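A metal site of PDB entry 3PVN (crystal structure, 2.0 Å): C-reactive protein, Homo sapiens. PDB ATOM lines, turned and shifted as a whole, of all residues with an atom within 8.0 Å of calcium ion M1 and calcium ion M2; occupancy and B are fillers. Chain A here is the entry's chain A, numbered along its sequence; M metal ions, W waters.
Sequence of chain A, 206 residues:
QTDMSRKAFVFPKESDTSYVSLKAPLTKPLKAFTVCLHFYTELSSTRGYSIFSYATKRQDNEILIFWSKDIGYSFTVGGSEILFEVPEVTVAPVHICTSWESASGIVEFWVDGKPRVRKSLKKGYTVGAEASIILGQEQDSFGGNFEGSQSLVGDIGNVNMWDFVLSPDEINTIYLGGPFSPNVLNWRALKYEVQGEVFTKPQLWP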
ATOM      1  N   SER A  50     -21.397 -27.939  20.502  1.00  0.00           N
ATOM      2  CA  SER A  50     -20.942 -28.315  19.189  1.00  0.00           C
ATOM      3  C   SER A  50     -19.404 -28.521  19.168  1.00  0.00           C
ATOM      4  O   SER A  50     -18.625 -27.703  19.741  1.00  0.00           O
ATOM      5  CB  SER A  50     -21.342 -27.233  18.214  1.00  0.00           C
ATOM      6  OG  SER A  50     -20.886 -27.539  16.919  1.00  0.00           O
ATOM      7  N   SER A  53     -18.756 -28.034  13.165  1.00  0.00           N
ATOM      8  CA  SER A  53     -20.019 -27.617  12.494  1.00  0.00           C
ATOM      9  C   SER A  53     -19.794 -27.210  11.036  1.00  0.00           C
ATOM     10  O   SER A  53     -19.117 -26.243  10.718  1.00  0.00           O
ATOM     11  CB  SER A  53     -20.663 -26.491  13.282  1.00  0.00           C
ATOM     12  OG  SER A  53     -21.841 -25.994  12.604  1.00  0.00           O
ATOM     13  N   TYR A  54     -20.347 -27.977  10.157  1.00  0.00           N
ATOM     14  CA  TYR A  54     -20.147 -27.805   8.699  1.00  0.00           C
ATOM     15  C   TYR A  54     -21.569 -27.599   8.095  1.00  0.00           C
ATOM     16  O   TYR A  54     -22.451 -28.456   8.223  1.00  0.00           O
ATOM     17  CB  TYR A  54     -19.454 -29.078   8.177  1.00  0.00           C
ATOM     18  CG  TYR A  54     -19.054 -29.234   6.721  1.00  0.00           C
ATOM     19  CD1 TYR A  54     -20.009 -29.404   5.714  1.00  0.00           C
ATOM     20  CD2 TYR A  54     -17.699 -29.338   6.370  1.00  0.00           C
ATOM     21  CE1 TYR A  54     -19.636 -29.555   4.403  1.00  0.00           C
ATOM     22  CE2 TYR A  54     -17.299 -29.516   5.046  1.00  0.00           C
ATOM     23  CZ  TYR A  54     -18.274 -29.603   4.073  1.00  0.00           C
ATOM     24  OH  TYR A  54     -17.866 -29.803   2.793  1.00  0.00           O
ATOM     25  N   ALA A  55     -21.767 -26.440   7.492  1.00  0.00           N
ATOM     26  CA  ALA A  55     -23.066 -26.081   6.957  1.00  0.00           C
ATOM     27  C   ALA A  55     -22.984 -25.716   5.478  1.00  0.00           C
ATOM     28  O   ALA A  55     -21.974 -25.170   5.027  1.00  0.00           O
ATOM     29  CB  ALA A  55     -23.667 -24.881   7.752  1.00  0.00           C
ATOM     30  N   GLN A  59     -28.328 -26.559   4.067  1.00  0.00           N
ATOM     31  CA  GLN A  59     -28.435 -27.484   5.215  1.00  0.00           C
ATOM     32  C   GLN A  59     -27.433 -27.046   6.310  1.00  0.00           C
ATOM     33  O   GLN A  59     -26.218 -27.057   6.070  1.00  0.00           O
ATOM     34  CB  GLN A  59     -28.183 -28.963   4.763  1.00  0.00           C
ATOM     35  CG  GLN A  59     -28.064 -29.953   5.942  1.00  0.00           C
ATOM     36  CD  GLN A  59     -29.334 -30.071   6.752  1.00  0.00           C
ATOM     37  OE1 GLN A  59     -29.421 -29.615   7.916  1.00  0.00           O
ATOM     38  NE2 GLN A  59     -30.315 -30.701   6.170  1.00  0.00           N
ATOM     39  N   ASP A  60     -27.950 -26.566   7.462  1.00  0.00           N
ATOM     40  CA  ASP A  60     -27.088 -26.013   8.535  1.00  0.00           C
ATOM     41  C   ASP A  60     -26.238 -27.119   9.167  1.00  0.00           C
ATOM     42  O   ASP A  60     -25.101 -26.878   9.560  1.00  0.00           O
ATOM     43  CB  ASP A  60     -27.899 -25.247   9.641  1.00  0.00           C
ATOM     44  CG  ASP A  60     -29.081 -26.024  10.134  1.00  0.00           C
ATOM     45  OD1 ASP A  60     -29.738 -26.658   9.281  1.00  0.00           O
ATOM     46  OD2 ASP A  60     -29.351 -26.032  11.357  1.00  0.00           O
ATOM     47  N   ASN A  61     -26.834 -28.293   9.270  1.00  0.00           N
ATOM     48  CA  ASN A  61     -26.192 -29.505   9.808  1.00  0.00           C
ATOM     49  C   ASN A  61     -25.766 -30.508   8.740  1.00  0.00           C
ATOM     50  O   ASN A  61     -26.192 -31.641   8.801  1.00  0.00           O
ATOM     51  CB  ASN A  61     -27.157 -30.136  10.802  1.00  0.00           C
ATOM     52  CG  ASN A  61     -27.498 -29.180  12.005  1.00  0.00           C
ATOM     53  OD1 ASN A  61     -26.860 -28.143  12.213  1.00  0.00           O
ATOM     54  ND2 ASN A  61     -28.476 -29.592  12.809  1.00  0.00           N
ATOM     55  N   GLU A  62     -24.980 -30.083   7.761  1.00  0.00           N
ATOM     56  CA  GLU A  62     -24.503 -30.941   6.647  1.00  0.00           C
ATOM     57  C   GLU A  62     -23.497 -31.967   7.225  1.00  0.00           C
ATOM     58  O   GLU A  62     -23.530 -33.150   6.818  1.00  0.00           O
ATOM     59  CB  GLU A  62     -23.860 -30.113   5.562  1.00  0.00           C
ATOM     60  CG  GLU A  62     -23.397 -30.916   4.318  1.00  0.00           C
ATOM     61  CD  GLU A  62     -24.555 -31.402   3.389  1.00  0.00           C
ATOM     62  OE1 GLU A  62     -25.695 -31.672   3.876  1.00  0.00           O
ATOM     63  OE2 GLU A  62     -24.294 -31.499   2.153  1.00  0.00           O
ATOM     64  N   LEU A  64     -22.239 -32.555  11.477  1.00  0.00           N
ATOM     65  CA  LEU A  64     -22.216 -31.964  12.813  1.00  0.00           C
ATOM     66  C   LEU A  64     -21.788 -33.006  13.841  1.00  0.00           C
ATOM     67  O   LEU A  64     -22.424 -34.035  13.970  1.00  0.00           O
ATOM     68  CB  LEU A  64     -23.620 -31.393  13.194  1.00  0.00           C
ATOM     69  CG  LEU A  64     -23.789 -30.884  14.654  1.00  0.00           C
ATOM     70  CD1 LEU A  64     -22.838 -29.741  14.932  1.00  0.00           C
ATOM     71  CD2 LEU A  64     -25.216 -30.336  14.904  1.00  0.00           C
ATOM     72  N   PHE A  66     -21.348 -33.364  17.843  1.00  0.00           N
ATOM     73  CA  PHE A  66     -21.961 -32.639  18.913  1.00  0.00           C
ATOM     74  C   PHE A  66     -21.925 -33.508  20.122  1.00  0.00           C
ATOM     75  O   PHE A  66     -22.000 -34.746  20.004  1.00  0.00           O
ATOM     76  CB  PHE A  66     -23.422 -32.281  18.497  1.00  0.00           C
ATOM     77  CG  PHE A  66     -24.145 -31.287  19.416  1.00  0.00           C
ATOM     78  CD1 PHE A  66     -24.098 -29.902  19.133  1.00  0.00           C
ATOM     79  CD2 PHE A  66     -24.889 -31.732  20.545  1.00  0.00           C
ATOM     80  CE1 PHE A  66     -24.724 -28.976  19.940  1.00  0.00           C
ATOM     81  CE2 PHE A  66     -25.578 -30.779  21.388  1.00  0.00           C
ATOM     82  CZ  PHE A  66     -25.481 -29.385  21.086  1.00  0.00           C
ATOM     83  N   GLN A 137     -18.756 -22.869  17.737  1.00  0.00           N
ATOM     84  CA  GLN A 137     -20.223 -22.573  17.756  1.00  0.00           C
ATOM     85  C   GLN A 137     -20.956 -23.533  16.819  1.00  0.00           C
ATOM     86  O   GLN A 137     -20.374 -24.071  15.867  1.00  0.00           O
ATOM     87  CB  GLN A 137     -20.558 -21.124  17.315  1.00  0.00           C
ATOM     88  CG  GLN A 137     -19.929 -19.958  18.047  1.00  0.00           C
ATOM     89  CD  GLN A 137     -20.399 -19.737  19.489  1.00  0.00           C
ATOM     90  OE1 GLN A 137     -19.630 -19.186  20.347  1.00  0.00           O
ATOM     91  NE2 GLN A 137     -21.598 -20.150  19.792  1.00  0.00           N
ATOM     92  N   GLU A 138     -22.244 -23.696  17.098  1.00  0.00           N
ATOM     93  CA  GLU A 138     -23.109 -24.537  16.307  1.00  0.00           C
ATOM     94  C   GLU A 138     -23.907 -23.652  15.358  1.00  0.00           C
ATOM     95  O   GLU A 138     -24.684 -22.788  15.824  1.00  0.00           O
ATOM     96  CB  GLU A 138     -24.041 -25.299  17.227  1.00  0.00           C
ATOM     97  CG  GLU A 138     -24.551 -26.578  16.604  1.00  0.00           C
ATOM     98  CD  GLU A 138     -25.544 -26.321  15.417  1.00  0.00           C
ATOM     99  OE1 GLU A 138     -26.623 -25.704  15.631  1.00  0.00           O
ATOM    100  OE2 GLU A 138     -25.202 -26.753  14.265  1.00  0.00           O
ATOM    101  N   GLN A 139     -23.726 -23.846  14.049  1.00  0.00           N
ATOM    102  CA  GLN A 139     -24.505 -23.097  12.991  1.00  0.00           C
ATOM    103  C   GLN A 139     -25.940 -23.475  12.813  1.00  0.00           C
ATOM    104  O   GLN A 139     -26.269 -24.648  12.616  1.00  0.00           O
ATOM    105  CB  GLN A 139     -23.842 -23.224  11.622  1.00  0.00           C
ATOM    106  CG  GLN A 139     -22.462 -22.615  11.568  1.00  0.00           C
ATOM    107  CD  GLN A 139     -21.739 -23.076  10.370  1.00  0.00           C
ATOM    108  OE1 GLN A 139     -21.276 -24.269  10.276  1.00  0.00           O
ATOM    109  NE2 GLN A 139     -21.646 -22.185   9.379  1.00  0.00           N
ATOM    110  N   ASP A 140     -26.823 -22.449  12.830  1.00  0.00           N
ATOM    111  CA  ASP A 140     -28.200 -22.608  12.414  1.00  0.00           C
ATOM    112  C   ASP A 140     -28.444 -21.937  11.049  1.00  0.00           C
ATOM    113  O   ASP A 140     -29.503 -22.069  10.481  1.00  0.00           O
ATOM    114  CB  ASP A 140     -29.177 -22.119  13.498  1.00  0.00           C
ATOM    115  CG  ASP A 140     -29.413 -23.143  14.581  1.00  0.00           C
ATOM    116  OD1 ASP A 140     -29.134 -24.349  14.385  1.00  0.00           O
ATOM    117  OD2 ASP A 140     -29.854 -22.781  15.698  1.00  0.00           O
ATOM    118  N   SER A 141     -27.461 -21.246  10.513  1.00  0.00           N
ATOM    119  CA  SER A 141     -27.518 -20.777   9.118  1.00  0.00           C
ATOM    120  C   SER A 141     -26.107 -20.819   8.577  1.00  0.00           C
ATOM    121  O   SER A 141     -25.173 -21.080   9.351  1.00  0.00           O
ATOM    122  CB  SER A 141     -28.085 -19.357   9.033  1.00  0.00           C
ATOM    123  OG  SER A 141     -27.149 -18.393   9.554  1.00  0.00           O
ATOM    124  N   GLY A 144     -23.562 -18.602  10.446  1.00  0.00           N
ATOM    125  CA  GLY A 144     -24.152 -17.762  11.487  1.00  0.00           C
ATOM    126  C   GLY A 144     -25.232 -18.372  12.333  1.00  0.00           C
ATOM    127  O   GLY A 144     -25.326 -19.569  12.465  1.00  0.00           O
ATOM    128  N   ASN A 145     -26.044 -17.516  12.930  1.00  0.00           N
ATOM    129  CA  ASN A 145     -27.084 -17.921  13.856  1.00  0.00           C
ATOM    130  C   ASN A 145     -26.619 -18.872  14.969  1.00  0.00           C
ATOM    131  O   ASN A 145     -27.136 -19.987  15.110  1.00  0.00           O
ATOM    132  CB  ASN A 145     -28.333 -18.438  13.125  1.00  0.00           C
ATOM    133  CG  ASN A 145     -29.217 -17.286  12.603  1.00  0.00           C
ATOM    134  OD1 ASN A 145     -28.996 -16.778  11.522  1.00  0.00           O
ATOM    135  ND2 ASN A 145     -30.183 -16.854  13.421  1.00  0.00           N
ATOM    136  N   PHE A 146     -25.668 -18.425  15.759  1.00  0.00           N
ATOM    137  CA  PHE A 146     -25.094 -19.237  16.839  1.00  0.00           C
ATOM    138  C   PHE A 146     -25.957 -19.218  18.138  1.00  0.00           C
ATOM    139  O   PHE A 146     -26.649 -18.252  18.402  1.00  0.00           O
ATOM    140  CB  PHE A 146     -23.657 -18.768  17.127  1.00  0.00           C
ATOM    141  CG  PHE A 146     -22.813 -18.627  15.885  1.00  0.00           C
ATOM    142  CD1 PHE A 146     -22.776 -19.652  14.940  1.00  0.00           C
ATOM    143  CD2 PHE A 146     -22.055 -17.479  15.650  1.00  0.00           C
ATOM    144  CE1 PHE A 146     -21.988 -19.538  13.779  1.00  0.00           C
ATOM    145  CE2 PHE A 146     -21.246 -17.358  14.517  1.00  0.00           C
ATOM    146  CZ  PHE A 146     -21.237 -18.394  13.551  1.00  0.00           C
ATOM    147  N   GLU A 147     -25.926 -20.289  18.928  1.00  0.00           N
ATOM    148  CA  GLU A 147     -26.570 -20.315  20.245  1.00  0.00           C
ATOM    149  C   GLU A 147     -25.492 -20.497  21.280  1.00  0.00           C
ATOM    150  O   GLU A 147     -24.722 -21.463  21.214  1.00  0.00           O
ATOM    151  CB  GLU A 147     -27.590 -21.447  20.368  1.00  0.00           C
ATOM    152  CG  GLU A 147     -28.801 -21.259  19.438  1.00  0.00           C
ATOM    153  CD  GLU A 147     -29.878 -22.375  19.554  1.00  0.00           C
ATOM    154  OE1 GLU A 147     -29.727 -23.489  18.960  1.00  0.00           O
ATOM    155  OE2 GLU A 147     -30.945 -22.086  20.173  1.00  0.00           O
ATOM    156  N   GLY A 148     -25.410 -19.559  22.237  1.00  0.00           N
ATOM    157  CA  GLY A 148     -24.452 -19.675  23.344  1.00  0.00           C
ATOM    158  C   GLY A 148     -24.586 -20.924  24.179  1.00  0.00           C
ATOM    159  O   GLY A 148     -23.620 -21.377  24.800  1.00  0.00           O
ATOM    160  N   SER A 149     -25.789 -21.490  24.232  1.00  0.00           N
ATOM    161  CA  SER A 149     -26.043 -22.699  25.015  1.00  0.00           C
ATOM    162  C   SER A 149     -25.443 -23.983  24.320  1.00  0.00           C
ATOM    163  O   SER A 149     -25.505 -25.065  24.891  1.00  0.00           O
ATOM    164  CB  SER A 149     -27.543 -22.876  25.239  1.00  0.00           C
ATOM    165  OG  SER A 149     -28.233 -23.198  24.014  1.00  0.00           O
ATOM    166  N   GLN A 150     -24.902 -23.819  23.113  1.00  0.00           N
ATOM    167  CA  GLN A 150     -24.214 -24.905  22.377  1.00  0.00           C
ATOM    168  C   GLN A 150     -22.746 -24.485  22.029  1.00  0.00           C
ATOM    169  O   GLN A 150     -22.074 -25.138  21.234  1.00  0.00           O
ATOM    170  CB  GLN A 150     -24.975 -25.245  21.078  1.00  0.00           C
ATOM    171  CG  GLN A 150     -26.480 -25.668  21.258  1.00  0.00           C
ATOM    172  CD  GLN A 150     -27.245 -25.780  19.908  1.00  0.00           C
ATOM    173  OE1 GLN A 150     -26.978 -25.035  18.978  1.00  0.00           O
ATOM    174  NE2 GLN A 150     -28.179 -26.738  19.818  1.00  0.00           N
HETATM  175 CA    CA M   1     -27.765 -26.229  13.581  1.00  0.00          CA
HETATM  176 CA    CA M   2     -28.252 -24.414  16.992  1.00  0.00          CA
HETATM  177  O   HOH W   1     -26.785 -22.224  16.777  1.00  0.00           O
HETATM  178  O   HOH W   2     -29.666 -27.447  15.925  1.00  0.00           O
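Five residues have an atom within 4 Å of calcium ion M1: Asp 60, Asn 61, Glu 138, Gln 139 and Asp 140. Along chain A the residues within 4 Å of calcium ion M1 span positions 60 to 140.
Calcium ion M1 is bound by the backbone carbonyl oxygen (O) of Gln 139 (2.4 Å), the side-chain carboxylate (OE1) of Glu 138 (2.4 Å), the side-chain carboxylate (OD1) of Asp 140 (2.5 Å), the side-chain amide oxygen (OD1) of Asn 61 (2.5 Å), the side-chain carboxylate (OE2) of Glu 138 (2.7 Å) and the side-chain carboxylate (OD2) of Asp 60 (2.7 Å).
The nearest printed residue that does not touch calcium ion M2 is Gln 139 (4.8 Å).
Calcium ion M2 is bound by OE1 of Gln 150. OE1 of Glu 138 is bound to calcium ion M2 (2.5 Å). Calcium ion M2 is bound by OE1 of Glu 147 (2.6 Å). Calcium ion M2 is bound by OD2 of Asp 140. Calcium ion M2 is bound by water W1 (2.6 Å). The side-chain carboxylate (OD1) of Asp 140 binds calcium ion M2, 2.8 Å away. Calcium ion M2 has six donor atoms within binding distance.
The side-chain hydroxyl (OG) of Ser 53 sits at hydrogen-bond distance from the side-chain amide oxygen (OE1) of Gln 139. O of Gln 150 sits at hydrogen-bond distance from N of Ser 50 (3.0 Å). The backbone NH (N) of Asp 140 sits close to the backbone carbonyl oxygen (O) of Asn 145, at 3.4 Å. N of Asn 61 lies within hydrogen-bond range of OE1 of Gln 59. The side-chain amide oxygen of Gln 59 sits close to the side-chain carboxylate of Asp 60, 3.3 Å away.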
